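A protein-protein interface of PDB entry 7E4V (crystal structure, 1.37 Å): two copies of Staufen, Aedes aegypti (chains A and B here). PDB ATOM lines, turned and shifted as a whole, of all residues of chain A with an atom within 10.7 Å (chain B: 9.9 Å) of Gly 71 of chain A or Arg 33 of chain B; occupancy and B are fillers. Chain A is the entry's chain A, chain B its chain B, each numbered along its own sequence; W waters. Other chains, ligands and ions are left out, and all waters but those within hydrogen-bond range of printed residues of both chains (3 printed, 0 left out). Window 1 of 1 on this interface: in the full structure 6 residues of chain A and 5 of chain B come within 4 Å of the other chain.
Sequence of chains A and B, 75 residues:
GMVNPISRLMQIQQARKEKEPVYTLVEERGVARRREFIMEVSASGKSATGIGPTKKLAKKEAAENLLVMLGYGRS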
ATOM      1  N   ARG A   8       1.695 -18.547 -11.555  1.00  0.00           N
ATOM      2  CA  ARG A   8       1.682 -18.134 -10.158  1.00  0.00           C
ATOM      3  C   ARG A   8       1.964 -19.316  -9.234  1.00  0.00           C
ATOM      4  O   ARG A   8       2.790 -19.224  -8.313  1.00  0.00           O
ATOM      5  CB  ARG A   8       0.332 -17.509  -9.839  1.00  0.00           C
ATOM      6  CG  ARG A   8       0.270 -16.921  -8.482  1.00  0.00           C
ATOM      7  CD  ARG A   8      -0.997 -16.128  -8.260  1.00  0.00           C
ATOM      8  NE  ARG A   8      -0.946 -15.586  -6.913  1.00  0.00           N
ATOM      9  CZ  ARG A   8      -1.848 -15.798  -5.965  1.00  0.00           C
ATOM     10  NH1 ARG A   8      -2.969 -16.464  -6.206  1.00  0.00           N
ATOM     11  NH2 ARG A   8      -1.608 -15.346  -4.741  1.00  0.00           N
ATOM     12  N   LEU A   9       1.292 -20.445  -9.474  1.00  0.00           N
ATOM     13  CA  LEU A   9       1.496 -21.629  -8.649  1.00  0.00           C
ATOM     14  C   LEU A   9       2.905 -22.181  -8.806  1.00  0.00           C
ATOM     15  O   LEU A   9       3.534 -22.567  -7.817  1.00  0.00           O
ATOM     16  CB  LEU A   9       0.453 -22.685  -9.009  1.00  0.00           C
ATOM     17  CG  LEU A   9       0.539 -24.019  -8.263  1.00  0.00           C
ATOM     18  CD1 LEU A   9       0.272 -23.859  -6.771  1.00  0.00           C
ATOM     19  CD2 LEU A   9      -0.426 -25.011  -8.884  1.00  0.00           C
ATOM     20  N   ILE A  12       5.260 -19.956  -6.793  1.00  0.00           N
ATOM     21  CA  ILE A  12       5.100 -20.144  -5.356  1.00  0.00           C
ATOM     22  C   ILE A  12       5.779 -21.430  -4.902  1.00  0.00           C
ATOM     23  O   ILE A  12       6.511 -21.438  -3.902  1.00  0.00           O
ATOM     24  CB  ILE A  12       3.616 -20.088  -4.972  1.00  0.00           C
ATOM     25  CG1 ILE A  12       3.153 -18.638  -5.038  1.00  0.00           C
ATOM     26  CG2 ILE A  12       3.389 -20.701  -3.575  1.00  0.00           C
ATOM     27  CD1 ILE A  12       1.662 -18.477  -4.858  1.00  0.00           C
ATOM     28  N   GLN A  13       5.588 -22.525  -5.648  1.00  0.00           N
ATOM     29  CA  GLN A  13       6.221 -23.786  -5.270  1.00  0.00           C
ATOM     30  C   GLN A  13       7.737 -23.685  -5.316  1.00  0.00           C
ATOM     31  O   GLN A  13       8.426 -24.201  -4.427  1.00  0.00           O
ATOM     32  CB  GLN A  13       5.716 -24.920  -6.164  1.00  0.00           C
ATOM     33  CG  GLN A  13       4.269 -25.307  -5.898  1.00  0.00           C
ATOM     34  CD  GLN A  13       4.019 -25.541  -4.418  1.00  0.00           C
ATOM     35  OE1 GLN A  13       3.442 -24.694  -3.737  1.00  0.00           O
ATOM     36  NE2 GLN A  13       4.465 -26.690  -3.916  1.00  0.00           N
ATOM     37  N   ALA A  15       9.542 -20.937  -4.851  1.00  0.00           N
ATOM     38  CA  ALA A  15       9.991 -20.110  -3.734  1.00  0.00           C
ATOM     39  C   ALA A  15       9.936 -20.864  -2.409  1.00  0.00           C
ATOM     40  O   ALA A  15      10.737 -20.581  -1.507  1.00  0.00           O
ATOM     41  CB  ALA A  15       9.156 -18.835  -3.662  1.00  0.00           C
ATOM     42  N   ARG A  16       8.994 -21.799  -2.264  1.00  0.00           N
ATOM     43  CA  ARG A  16       8.896 -22.634  -1.069  1.00  0.00           C
ATOM     44  C   ARG A  16       9.874 -23.795  -1.078  1.00  0.00           C
ATOM     45  O   ARG A  16       9.913 -24.555  -0.105  1.00  0.00           O
ATOM     46  CB  ARG A  16       7.469 -23.160  -0.916  1.00  0.00           C
ATOM     47  CG  ARG A  16       6.457 -22.054  -0.693  1.00  0.00           C
ATOM     48  CD  ARG A  16       5.021 -22.555  -0.697  1.00  0.00           C
ATOM     49  NE  ARG A  16       4.840 -23.608   0.293  1.00  0.00           N
ATOM     50  CZ  ARG A  16       4.543 -23.391   1.565  1.00  0.00           C
ATOM     51  NH1 ARG A  16       4.310 -22.173   2.025  1.00  0.00           N
ATOM     52  NH2 ARG A  16       4.514 -24.422   2.406  1.00  0.00           N
ATOM     53  N   GLU A  18       9.603 -26.443  -2.775  1.00  0.00           N
ATOM     54  CA  GLU A  18       8.773 -27.636  -2.803  1.00  0.00           C
ATOM     55  C   GLU A  18       8.748 -28.235  -4.209  1.00  0.00           C
ATOM     56  O   GLU A  18       9.199 -27.622  -5.185  1.00  0.00           O
ATOM     57  CB  GLU A  18       7.354 -27.279  -2.320  1.00  0.00           C
ATOM     58  CG  GLU A  18       7.297 -27.048  -0.799  1.00  0.00           C
ATOM     59  CD  GLU A  18       5.918 -26.723  -0.230  1.00  0.00           C
ATOM     60  OE1 GLU A  18       4.938 -26.521  -0.981  1.00  0.00           O
ATOM     61  OE2 GLU A  18       5.806 -26.672   1.016  1.00  0.00           O
ATOM     62  N   ALA A  43      -0.169 -30.208  -5.698  1.00  0.00           N
ATOM     63  CA  ALA A  43       1.018 -29.511  -5.214  1.00  0.00           C
ATOM     64  C   ALA A  43       0.832 -29.219  -3.737  1.00  0.00           C
ATOM     65  O   ALA A  43      -0.290 -29.011  -3.280  1.00  0.00           O
ATOM     66  CB  ALA A  43       1.268 -28.195  -5.963  1.00  0.00           C
ATOM     67  N   SER A  44       1.944 -29.218  -2.996  1.00  0.00           N
ATOM     68  CA  SER A  44       1.956 -28.790  -1.599  1.00  0.00           C
ATOM     69  C   SER A  44       0.977 -29.585  -0.738  1.00  0.00           C
ATOM     70  O   SER A  44       0.354 -29.040   0.171  1.00  0.00           O
ATOM     71  CB  SER A  44       1.682 -27.284  -1.497  1.00  0.00           C
ATOM     72  OG  SER A  44       2.291 -26.693  -0.352  1.00  0.00           O
ATOM     73  N   GLY A  45       0.793 -30.866  -1.045  1.00  0.00           N
ATOM     74  CA  GLY A  45      -0.029 -31.733  -0.230  1.00  0.00           C
ATOM     75  C   GLY A  45      -1.514 -31.693  -0.518  1.00  0.00           C
ATOM     76  O   GLY A  45      -2.282 -32.341   0.203  1.00  0.00           O
ATOM     77  N   LYS A  46      -1.953 -30.959  -1.540  1.00  0.00           N
ATOM     78  CA  LYS A  46      -3.363 -30.850  -1.876  1.00  0.00           C
ATOM     79  C   LYS A  46      -3.540 -31.059  -3.372  1.00  0.00           C
ATOM     80  O   LYS A  46      -2.586 -31.020  -4.152  1.00  0.00           O
ATOM     81  CB  LYS A  46      -3.942 -29.483  -1.468  1.00  0.00           C
ATOM     82  CG  LYS A  46      -4.040 -29.285   0.051  1.00  0.00           C
ATOM     83  CD  LYS A  46      -4.936 -28.123   0.402  1.00  0.00           C
ATOM     84  CE  LYS A  46      -5.210 -28.109   1.897  1.00  0.00           C
ATOM     85  NZ  LYS A  46      -5.930 -26.872   2.329  1.00  0.00           N
ATOM     86  N   SER A  47      -4.783 -31.287  -3.774  1.00  0.00           N
ATOM     87  CA  SER A  47      -5.097 -31.449  -5.180  1.00  0.00           C
ATOM     88  C   SER A  47      -6.413 -30.745  -5.480  1.00  0.00           C
ATOM     89  O   SER A  47      -7.226 -30.505  -4.590  1.00  0.00           O
ATOM     90  CB  SER A  47      -5.121 -32.924  -5.576  1.00  0.00           C
ATOM     91  OG  SER A  47      -6.185 -33.598  -4.948  1.00  0.00           O
ATOM     92  N   ALA A  48      -6.606 -30.373  -6.740  1.00  0.00           N
ATOM     93  CA  ALA A  48      -7.840 -29.720  -7.146  1.00  0.00           C
ATOM     94  C   ALA A  48      -8.094 -30.041  -8.603  1.00  0.00           C
ATOM     95  O   ALA A  48      -7.180 -30.404  -9.348  1.00  0.00           O
ATOM     96  CB  ALA A  48      -7.779 -28.197  -6.949  1.00  0.00           C
ATOM     97  N   ALA A  63      -5.348 -24.884 -11.521  1.00  0.00           N
ATOM     98  CA  ALA A  63      -4.331 -24.176 -10.747  1.00  0.00           C
ATOM     99  C   ALA A  63      -4.962 -23.108  -9.874  1.00  0.00           C
ATOM    100  O   ALA A  63      -4.579 -22.941  -8.709  1.00  0.00           O
ATOM    101  CB  ALA A  63      -3.286 -23.561 -11.682  1.00  0.00           C
ATOM    102  N   GLU A  64      -5.939 -22.381 -10.410  1.00  0.00           N
ATOM    103  CA  GLU A  64      -6.621 -21.359  -9.629  1.00  0.00           C
ATOM    104  C   GLU A  64      -7.316 -21.976  -8.420  1.00  0.00           C
ATOM    105  O   GLU A  64      -7.217 -21.462  -7.297  1.00  0.00           O
ATOM    106  CB  GLU A  64      -7.643 -20.656 -10.519  1.00  0.00           C
ATOM    107  CG  GLU A  64      -8.525 -19.618  -9.835  1.00  0.00           C
ATOM    108  CD  GLU A  64      -7.776 -18.402  -9.324  1.00  0.00           C
ATOM    109  OE1 GLU A  64      -8.447 -17.404  -8.979  1.00  0.00           O
ATOM    110  OE2 GLU A  64      -6.524 -18.378  -9.333  1.00  0.00           O
ATOM    111  N   ASN A  65      -8.011 -23.100  -8.617  1.00  0.00           N
ATOM    112  CA  ASN A  65      -8.713 -23.743  -7.510  1.00  0.00           C
ATOM    113  C   ASN A  65      -7.738 -24.272  -6.466  1.00  0.00           C
ATOM    114  O   ASN A  65      -8.033 -24.242  -5.260  1.00  0.00           O
ATOM    115  CB  ASN A  65      -9.615 -24.860  -8.053  1.00  0.00           C
ATOM    116  CG  ASN A  65     -10.814 -24.319  -8.792  1.00  0.00           C
ATOM    117  OD1 ASN A  65     -11.239 -23.189  -8.553  1.00  0.00           O
ATOM    118  ND2 ASN A  65     -11.368 -25.115  -9.703  1.00  0.00           N
ATOM    119  N   LEU A  66      -6.571 -24.767  -6.898  1.00  0.00           N
ATOM    120  CA  LEU A  66      -5.575 -25.234  -5.944  1.00  0.00           C
ATOM    121  C   LEU A  66      -4.968 -24.074  -5.168  1.00  0.00           C
ATOM    122  O   LEU A  66      -4.786 -24.168  -3.943  1.00  0.00           O
ATOM    123  CB  LEU A  66      -4.501 -26.064  -6.640  1.00  0.00           C
ATOM    124  CG  LEU A  66      -3.483 -26.644  -5.660  1.00  0.00           C
ATOM    125  CD1 LEU A  66      -4.174 -27.498  -4.611  1.00  0.00           C
ATOM    126  CD2 LEU A  66      -2.456 -27.445  -6.421  1.00  0.00           C
ATOM    127  N   LEU A  67      -4.680 -22.958  -5.845  1.00  0.00           N
ATOM    128  CA  LEU A  67      -4.150 -21.791  -5.139  1.00  0.00           C
ATOM    129  C   LEU A  67      -5.115 -21.326  -4.054  1.00  0.00           C
ATOM    130  O   LEU A  67      -4.698 -20.975  -2.940  1.00  0.00           O
ATOM    131  CB  LEU A  67      -3.876 -20.666  -6.129  1.00  0.00           C
ATOM    132  CG  LEU A  67      -2.622 -20.798  -6.994  1.00  0.00           C
ATOM    133  CD1 LEU A  67      -2.743 -19.914  -8.224  1.00  0.00           C
ATOM    134  CD2 LEU A  67      -1.392 -20.401  -6.197  1.00  0.00           C
ATOM    135  N   VAL A  68      -6.414 -21.337  -4.353  1.00  0.00           N
ATOM    136  CA  VAL A  68      -7.414 -20.971  -3.356  1.00  0.00           C
ATOM    137  C   VAL A  68      -7.417 -21.965  -2.201  1.00  0.00           C
ATOM    138  O   VAL A  68      -7.429 -21.574  -1.026  1.00  0.00           O
ATOM    139  CB  VAL A  68      -8.796 -20.827  -4.015  1.00  0.00           C
ATOM    140  CG1 VAL A  68      -9.888 -20.801  -2.964  1.00  0.00           C
ATOM    141  CG2 VAL A  68      -8.845 -19.550  -4.840  1.00  0.00           C
ATOM    142  N   MET A  69      -7.383 -23.264  -2.512  1.00  0.00           N
ATOM    143  CA  MET A  69      -7.369 -24.281  -1.462  1.00  0.00           C
ATOM    144  C   MET A  69      -6.152 -24.130  -0.561  1.00  0.00           C
ATOM    145  O   MET A  69      -6.225 -24.389   0.645  1.00  0.00           O
ATOM    146  CB  MET A  69      -7.307 -25.669  -2.092  1.00  0.00           C
ATOM    147  CG  MET A  69      -8.590 -26.275  -2.575  1.00  0.00           C
ATOM    148  SD  MET A  69      -8.173 -27.931  -3.187  1.00  0.00           S
ATOM    149  CE  MET A  69      -7.909 -28.861  -1.692  1.00  0.00           C
ATOM    150  N   LEU A  70      -5.013 -23.738  -1.130  1.00  0.00           N
ATOM    151  CA  LEU A  70      -3.766 -23.596  -0.392  1.00  0.00           C
ATOM    152  C   LEU A  70      -3.669 -22.283   0.374  1.00  0.00           C
ATOM    153  O   LEU A  70      -2.686 -22.086   1.097  1.00  0.00           O
ATOM    154  CB  LEU A  70      -2.565 -23.753  -1.346  1.00  0.00           C
ATOM    155  CG  LEU A  70      -2.316 -25.175  -1.859  1.00  0.00           C
ATOM    156  CD1 LEU A  70      -1.307 -25.167  -2.993  1.00  0.00           C
ATOM    157  CD2 LEU A  70      -1.820 -26.079  -0.748  1.00  0.00           C
ATOM    158  N   GLY A  71      -4.658 -21.404   0.275  1.00  0.00           N
ATOM    159  CA  GLY A  71      -4.649 -20.185   1.059  1.00  0.00           C
ATOM    160  C   GLY A  71      -3.986 -18.993   0.421  1.00  0.00           C
ATOM    161  O   GLY A  71      -3.700 -18.018   1.120  1.00  0.00           O
ATOM    162  N   TYR A  72      -3.735 -19.022  -0.879  1.00  0.00           N
ATOM    163  CA  TYR A  72      -3.072 -17.917  -1.558  1.00  0.00           C
ATOM    164  C   TYR A  72      -4.048 -16.950  -2.218  1.00  0.00           C
ATOM    165  O   TYR A  72      -3.611 -15.976  -2.845  1.00  0.00           O
ATOM    166  CB  TYR A  72      -2.067 -18.458  -2.578  1.00  0.00           C
ATOM    167  CG  TYR A  72      -0.968 -19.288  -1.943  1.00  0.00           C
ATOM    168  CD1 TYR A  72      -0.154 -18.779  -0.940  1.00  0.00           C
ATOM    169  CD2 TYR A  72      -0.809 -20.617  -2.300  1.00  0.00           C
ATOM    170  CE1 TYR A  72       0.839 -19.573  -0.352  1.00  0.00           C
ATOM    171  CE2 TYR A  72       0.145 -21.408  -1.725  1.00  0.00           C
ATOM    172  CZ  TYR A  72       0.978 -20.887  -0.757  1.00  0.00           C
ATOM    173  OH  TYR A  72       1.954 -21.676  -0.186  1.00  0.00           O
ATOM    174  N   GLY A  73      -5.347 -17.194  -2.100  1.00  0.00           N
ATOM    175  CA  GLY A  73      -6.346 -16.295  -2.631  1.00  0.00           C
ATOM    176  C   GLY A  73      -6.557 -16.463  -4.121  1.00  0.00           C
ATOM    177  O   GLY A  73      -5.800 -17.129  -4.837  1.00  0.00           O
ATOM    178  N   ARG A  74      -7.633 -15.833  -4.591  1.00  0.00           N
ATOM    179  CA  ARG A  74      -7.978 -15.871  -6.001  1.00  0.00           C
ATOM    180  C   ARG A  74      -6.978 -15.061  -6.819  1.00  0.00           C
ATOM    181  O   ARG A  74      -6.338 -14.131  -6.320  1.00  0.00           O
ATOM    182  CB  ARG A  74      -9.383 -15.313  -6.209  1.00  0.00           C
ATOM    183  CG  ARG A  74     -10.470 -16.283  -5.797  1.00  0.00           C
ATOM    184  CD  ARG A  74     -11.831 -15.602  -5.769  1.00  0.00           C
ATOM    185  NE  ARG A  74     -11.876 -14.508  -4.808  1.00  0.00           N
ATOM    186  CZ  ARG A  74     -12.876 -13.642  -4.712  1.00  0.00           C
ATOM    187  NH1 ARG A  74     -13.927 -13.716  -5.509  1.00  0.00           N
ATOM    188  NH2 ARG A  74     -12.818 -12.682  -3.794  1.00  0.00           N
ATOM    189  N   SER A  75      -6.884 -15.424  -8.101  1.00  0.00           N
ATOM    190  CA  SER A  75      -5.902 -14.921  -9.068  1.00  0.00           C
ATOM    191  C   SER A  75      -4.492 -15.430  -8.773  1.00  0.00           C
ATOM    192  O   SER A  75      -4.231 -16.642  -8.843  1.00  0.00           O
ATOM    193  CB  SER A  75      -5.942 -13.396  -9.184  1.00  0.00           C
ATOM    194  N   ARG B  29     -11.831 -14.546   9.206  1.00  0.00           N
ATOM    195  CA  ARG B  29     -10.817 -14.674  10.232  1.00  0.00           C
ATOM    196  C   ARG B  29      -9.602 -15.406   9.691  1.00  0.00           C
ATOM    197  O   ARG B  29      -9.660 -16.083   8.664  1.00  0.00           O
ATOM    198  CB  ARG B  29     -11.374 -15.427  11.437  1.00  0.00           C
ATOM    199  CG  ARG B  29     -11.850 -16.815  11.091  1.00  0.00           C
ATOM    200  CD  ARG B  29     -12.713 -17.394  12.197  1.00  0.00           C
ATOM    201  NE  ARG B  29     -11.916 -17.873  13.321  1.00  0.00           N
ATOM    202  CZ  ARG B  29     -12.373 -17.972  14.560  1.00  0.00           C
ATOM    203  NH1 ARG B  29     -13.608 -17.620  14.865  1.00  0.00           N
ATOM    204  NH2 ARG B  29     -11.573 -18.433  15.516  1.00  0.00           N
ATOM    205  N   GLY B  30      -8.507 -15.309  10.425  1.00  0.00           N
ATOM    206  CA  GLY B  30      -7.306 -16.041  10.087  1.00  0.00           C
ATOM    207  C   GLY B  30      -6.227 -15.173   9.475  1.00  0.00           C
ATOM    208  O   GLY B  30      -6.493 -14.153   8.821  1.00  0.00           O
ATOM    209  N   VAL B  31      -4.984 -15.598   9.673  1.00  0.00           N
ATOM    210  CA  VAL B  31      -3.794 -14.889   9.222  1.00  0.00           C
ATOM    211  C   VAL B  31      -3.236 -15.607   8.003  1.00  0.00           C
ATOM    212  O   VAL B  31      -3.161 -16.838   7.976  1.00  0.00           O
ATOM    213  CB  VAL B  31      -2.765 -14.838  10.370  1.00  0.00           C
ATOM    214  CG1 VAL B  31      -1.456 -14.235   9.895  1.00  0.00           C
ATOM    215  CG2 VAL B  31      -3.341 -14.044  11.543  1.00  0.00           C
ATOM    216  N   ALA B  32      -2.858 -14.833   6.982  1.00  0.00           N
ATOM    217  CA  ALA B  32      -2.078 -15.327   5.839  1.00  0.00           C
ATOM    218  C   ALA B  32      -2.786 -16.504   5.178  1.00  0.00           C
ATOM    219  O   ALA B  32      -3.954 -16.359   4.767  1.00  0.00           O
ATOM    220  CB  ALA B  32      -0.628 -15.561   6.267  1.00  0.00           C
ATOM    221  N   ARG B  33      -2.158 -17.673   5.070  1.00  0.00           N
ATOM    222  CA  ARG B  33      -2.751 -18.797   4.357  1.00  0.00           C
ATOM    223  C   ARG B  33      -3.950 -19.393   5.071  1.00  0.00           C
ATOM    224  O   ARG B  33      -4.660 -20.210   4.472  1.00  0.00           O
ATOM    225  CB  ARG B  33      -1.706 -19.899   4.140  1.00  0.00           C
ATOM    226  CG  ARG B  33      -0.584 -19.491   3.200  1.00  0.00           C
ATOM    227  CD  ARG B  33       0.425 -20.616   3.067  1.00  0.00           C
ATOM    228  NE  ARG B  33      -0.211 -21.770   2.460  1.00  0.00           N
ATOM    229  CZ  ARG B  33       0.230 -23.010   2.562  1.00  0.00           C
ATOM    230  NH1 ARG B  33       1.332 -23.299   3.239  1.00  0.00           N
ATOM    231  NH2 ARG B  33      -0.452 -23.990   1.972  1.00  0.00           N
ATOM    232  N   ARG B  34      -4.211 -18.996   6.314  1.00  0.00           N
ATOM    233  CA  ARG B  34      -5.326 -19.515   7.088  1.00  0.00           C
ATOM    234  C   ARG B  34      -6.561 -18.632   7.008  1.00  0.00           C
ATOM    235  O   ARG B  34      -7.544 -18.899   7.711  1.00  0.00           O
ATOM    236  CB  ARG B  34      -4.918 -19.701   8.544  1.00  0.00           C
ATOM    237  N   ARG B  35      -6.547 -17.595   6.174  1.00  0.00           N
ATOM    238  CA  ARG B  35      -7.716 -16.734   6.049  1.00  0.00           C
ATOM    239  C   ARG B  35      -8.902 -17.537   5.541  1.00  0.00           C
ATOM    240  O   ARG B  35      -8.801 -18.284   4.560  1.00  0.00           O
ATOM    241  CB  ARG B  35      -7.411 -15.611   5.062  1.00  0.00           C
ATOM    242  CG  ARG B  35      -8.344 -14.411   5.197  1.00  0.00           C
ATOM    243  CD  ARG B  35      -8.081 -13.375   4.117  1.00  0.00           C
ATOM    244  NE  ARG B  35      -7.556 -13.989   2.903  1.00  0.00           N
ATOM    245  CZ  ARG B  35      -8.220 -14.084   1.758  1.00  0.00           C
ATOM    246  NH1 ARG B  35      -9.443 -13.596   1.625  1.00  0.00           N
ATOM    247  NH2 ARG B  35      -7.637 -14.681   0.719  1.00  0.00           N
ATOM    248  N   GLU B  36     -10.034 -17.379   6.215  1.00  0.00           N
ATOM    249  CA  GLU B  36     -11.243 -18.092   5.844  1.00  0.00           C
ATOM    250  C   GLU B  36     -12.466 -17.252   6.162  1.00  0.00           C
ATOM    251  O   GLU B  36     -12.409 -16.259   6.892  1.00  0.00           O
ATOM    252  CB  GLU B  36     -11.318 -19.439   6.537  1.00  0.00           C
ATOM    253  CG  GLU B  36     -11.426 -19.319   8.016  1.00  0.00           C
ATOM    254  CD  GLU B  36     -11.453 -20.665   8.684  1.00  0.00           C
ATOM    255  OE1 GLU B  36     -11.747 -20.724   9.895  1.00  0.00           O
ATOM    256  OE2 GLU B  36     -11.134 -21.657   7.997  1.00  0.00           O
ATOM    257  N   PHE B  37     -13.570 -17.656   5.555  1.00  0.00           N
ATOM    258  CA  PHE B  37     -14.869 -17.041   5.735  1.00  0.00           C
ATOM    259  C   PHE B  37     -15.820 -18.018   6.404  1.00  0.00           C
ATOM    260  O   PHE B  37     -15.793 -19.217   6.114  1.00  0.00           O
ATOM    261  CB  PHE B  37     -15.439 -16.650   4.375  1.00  0.00           C
ATOM    262  CG  PHE B  37     -14.663 -15.570   3.688  1.00  0.00           C
ATOM    263  CD1 PHE B  37     -13.520 -15.874   2.972  1.00  0.00           C
ATOM    264  CD2 PHE B  37     -15.062 -14.251   3.777  1.00  0.00           C
ATOM    265  CE1 PHE B  37     -12.788 -14.877   2.337  1.00  0.00           C
ATOM    266  CE2 PHE B  37     -14.337 -13.247   3.147  1.00  0.00           C
ATOM    267  CZ  PHE B  37     -13.207 -13.564   2.426  1.00  0.00           C
ATOM    268  N   GLY B  52     -15.080 -21.731   4.457  1.00  0.00           N
ATOM    269  CA  GLY B  52     -14.279 -21.919   3.267  1.00  0.00           C
ATOM    270  C   GLY B  52     -13.290 -20.792   3.042  1.00  0.00           C
ATOM    271  O   GLY B  52     -13.377 -19.732   3.667  1.00  0.00           O
ATOM    272  N   PRO B  53     -12.340 -20.988   2.120  1.00  0.00           N
ATOM    273  CA  PRO B  53     -11.321 -19.954   1.868  1.00  0.00           C
ATOM    274  C   PRO B  53     -11.806 -18.784   1.036  1.00  0.00           C
ATOM    275  O   PRO B  53     -11.085 -17.781   0.937  1.00  0.00           O
ATOM    276  CB  PRO B  53     -10.199 -20.712   1.144  1.00  0.00           C
ATOM    277  CG  PRO B  53     -10.823 -21.984   0.642  1.00  0.00           C
ATOM    278  CD  PRO B  53     -12.135 -22.218   1.336  1.00  0.00           C
ATOM    279  N   THR B  54     -12.990 -18.874   0.440  1.00  0.00           N
ATOM    280  CA  THR B  54     -13.634 -17.727  -0.182  1.00  0.00           C
ATOM    281  C   THR B  54     -15.064 -17.654   0.321  1.00  0.00           C
ATOM    282  O   THR B  54     -15.614 -18.623   0.855  1.00  0.00           O
ATOM    283  CB  THR B  54     -13.695 -17.825  -1.708  1.00  0.00           C
ATOM    284  OG1 THR B  54     -14.560 -18.902  -2.079  1.00  0.00           O
ATOM    285  CG2 THR B  54     -12.314 -18.028  -2.321  1.00  0.00           C
ATOM    286  N   LEU B  57     -17.231 -20.260  -1.534  1.00  0.00           N
ATOM    287  CA  LEU B  57     -17.051 -21.625  -1.051  1.00  0.00           C
ATOM    288  C   LEU B  57     -17.698 -21.826   0.312  1.00  0.00           C
ATOM    289  O   LEU B  57     -18.284 -22.883   0.577  1.00  0.00           O
ATOM    290  CB  LEU B  57     -15.569 -21.993  -1.007  1.00  0.00           C
ATOM    291  CG  LEU B  57     -14.925 -22.232  -2.373  1.00  0.00           C
ATOM    292  CD1 LEU B  57     -13.405 -22.254  -2.248  1.00  0.00           C
ATOM    293  CD2 LEU B  57     -15.427 -23.537  -2.977  1.00  0.00           C
HETATM  294  O   HOH W   1       1.030 -26.454   2.109  1.00  0.00           O
HETATM  295  O   HOH W   2     -11.400 -14.205  -1.080  1.00  0.00           O
HETATM  296  O   HOH W   3      -3.656 -25.056   2.750  1.00  0.00           O
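NE of Arg 33 of chain B sits at hydrogen-bond distance from O of Leu 70 of chain A.
The side-chain hydroxyl (OH) of Tyr 72 of chain A lies within hydrogen-bond range of the guanidinium group (NE) of Arg 33 of chain B (3.4 Å).
The guanidinium group (NH1) of Arg 16 of chain A sits close to the guanidinium group (NH1) of Arg 33 of chain B.
NH2 of Arg 8 of chain A sits at hydrogen-bond distance from O of Tyr 72 of chain A, 2.8 Å away.
The guanidinium group (NH1) of Arg 8 of chain A sits at hydrogen-bond distance from the backbone carbonyl oxygen (O) of Gly 73 of chain A (3.2 Å).
NH2 of Arg 16 of chain A is in salt-bridge range of OE2 of Glu 18 of chain A, at 2.9 Å.
The guanidinium group of Arg 16 of chain A sits close to the side-chain hydroxyl of Tyr 72 of chain A.
O of Leu 67 of chain A is in hydrogen-bond range of N of Tyr 72 of chain A, 3.0 Å away.
The side-chain hydroxyl of Thr 54 of chain B sits at hydrogen-bond distance from the backbone NH of Leu 57 of chain B (3.0 Å).
Among the printed residues, merely in contact across the chains: Gly 71 of chain A with Arg 33 of chain B, Val 68 of chain A with Pro 53 of chain B, Val 68 of chain A with Thr 54 of chain B, Val 68 of chain A with Leu 57 of chain B and Gly 73 of chain A with Arg 35 of chain B.
Printed residues of chain B within 4 Å of Gly 71 of chain A: Arg 33.
Arg 33 of chain B touches just these residues of chain A: Arg 16 (3.4 Å), Leu 70 (2.8 Å), Gly 71 (3.4 Å) and Tyr 72 (3.4 Å).
Of chain B, only Arg 33 comes within 4 Å of Leu 70 of chain A.
Of the printed residues of chain B, Tyr 72 of chain A touches Arg 33.
No residue of chain A comes within 4 Å of Arg 34 of chain B.
Printed residues of chain B within 4 Å of Arg 16 of chain A: Arg 33 (3.4 Å).
Printed residues of chain A within 4 Å of Pro 53 of chain B: Val 68 (3.6 Å).
Of the printed residues of chain A, Thr 54 of chain B touches Val 68 (3.7 Å).
Of the printed residues of chain B, Val 68 of chain A touches Pro 53, Thr 54 and Leu 57.
Glu 36 of chain B touches none of the printed residues of chain A.
Of the 13 printed residues of chain B, 5 touch a printed residue of chain A.
Printed residues of chain B that touch a printed residue of chain A: Arg 33, Arg 35, Pro 53, Thr 54 and Leu 57.
Hydrophobic or aromatic side chains of chain B within 4 Å of the printed part of chain A: Pro 53 and Leu 57.
Hydrophobic or aromatic side chains of chain A that line the printed part of chain B: Val 68, Leu 70 and Tyr 72.
Among the printed residues, no Asp or Glu carboxylate lies within 4 Å of a Lys or Arg side-chain nitrogen of the other chain.
No position is printed for both chains.
Of the 8 pairs that touch across the chains among the printed residues, none has its exchanged pair printed and touching as well.
Water W1 lies within hydrogen-bond range of OG of Ser 44 of chain A and NH2 of Arg 33 of chain B.
Water W3 lies within hydrogen-bond range of the side-chain amino group (NZ) of Lys 46 of chain A (2.9 Å), the backbone carbonyl oxygen (O) of Met 69 of chain A (3.4 Å) and the guanidinium group (NH2) of Arg 33 of chain B (3.5 Å).
Water W2 lies within hydrogen-bond range of NH1 of Arg 35 of chain B (3.4 Å) and NH2 of Arg 74 of chain A (3.4 Å).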
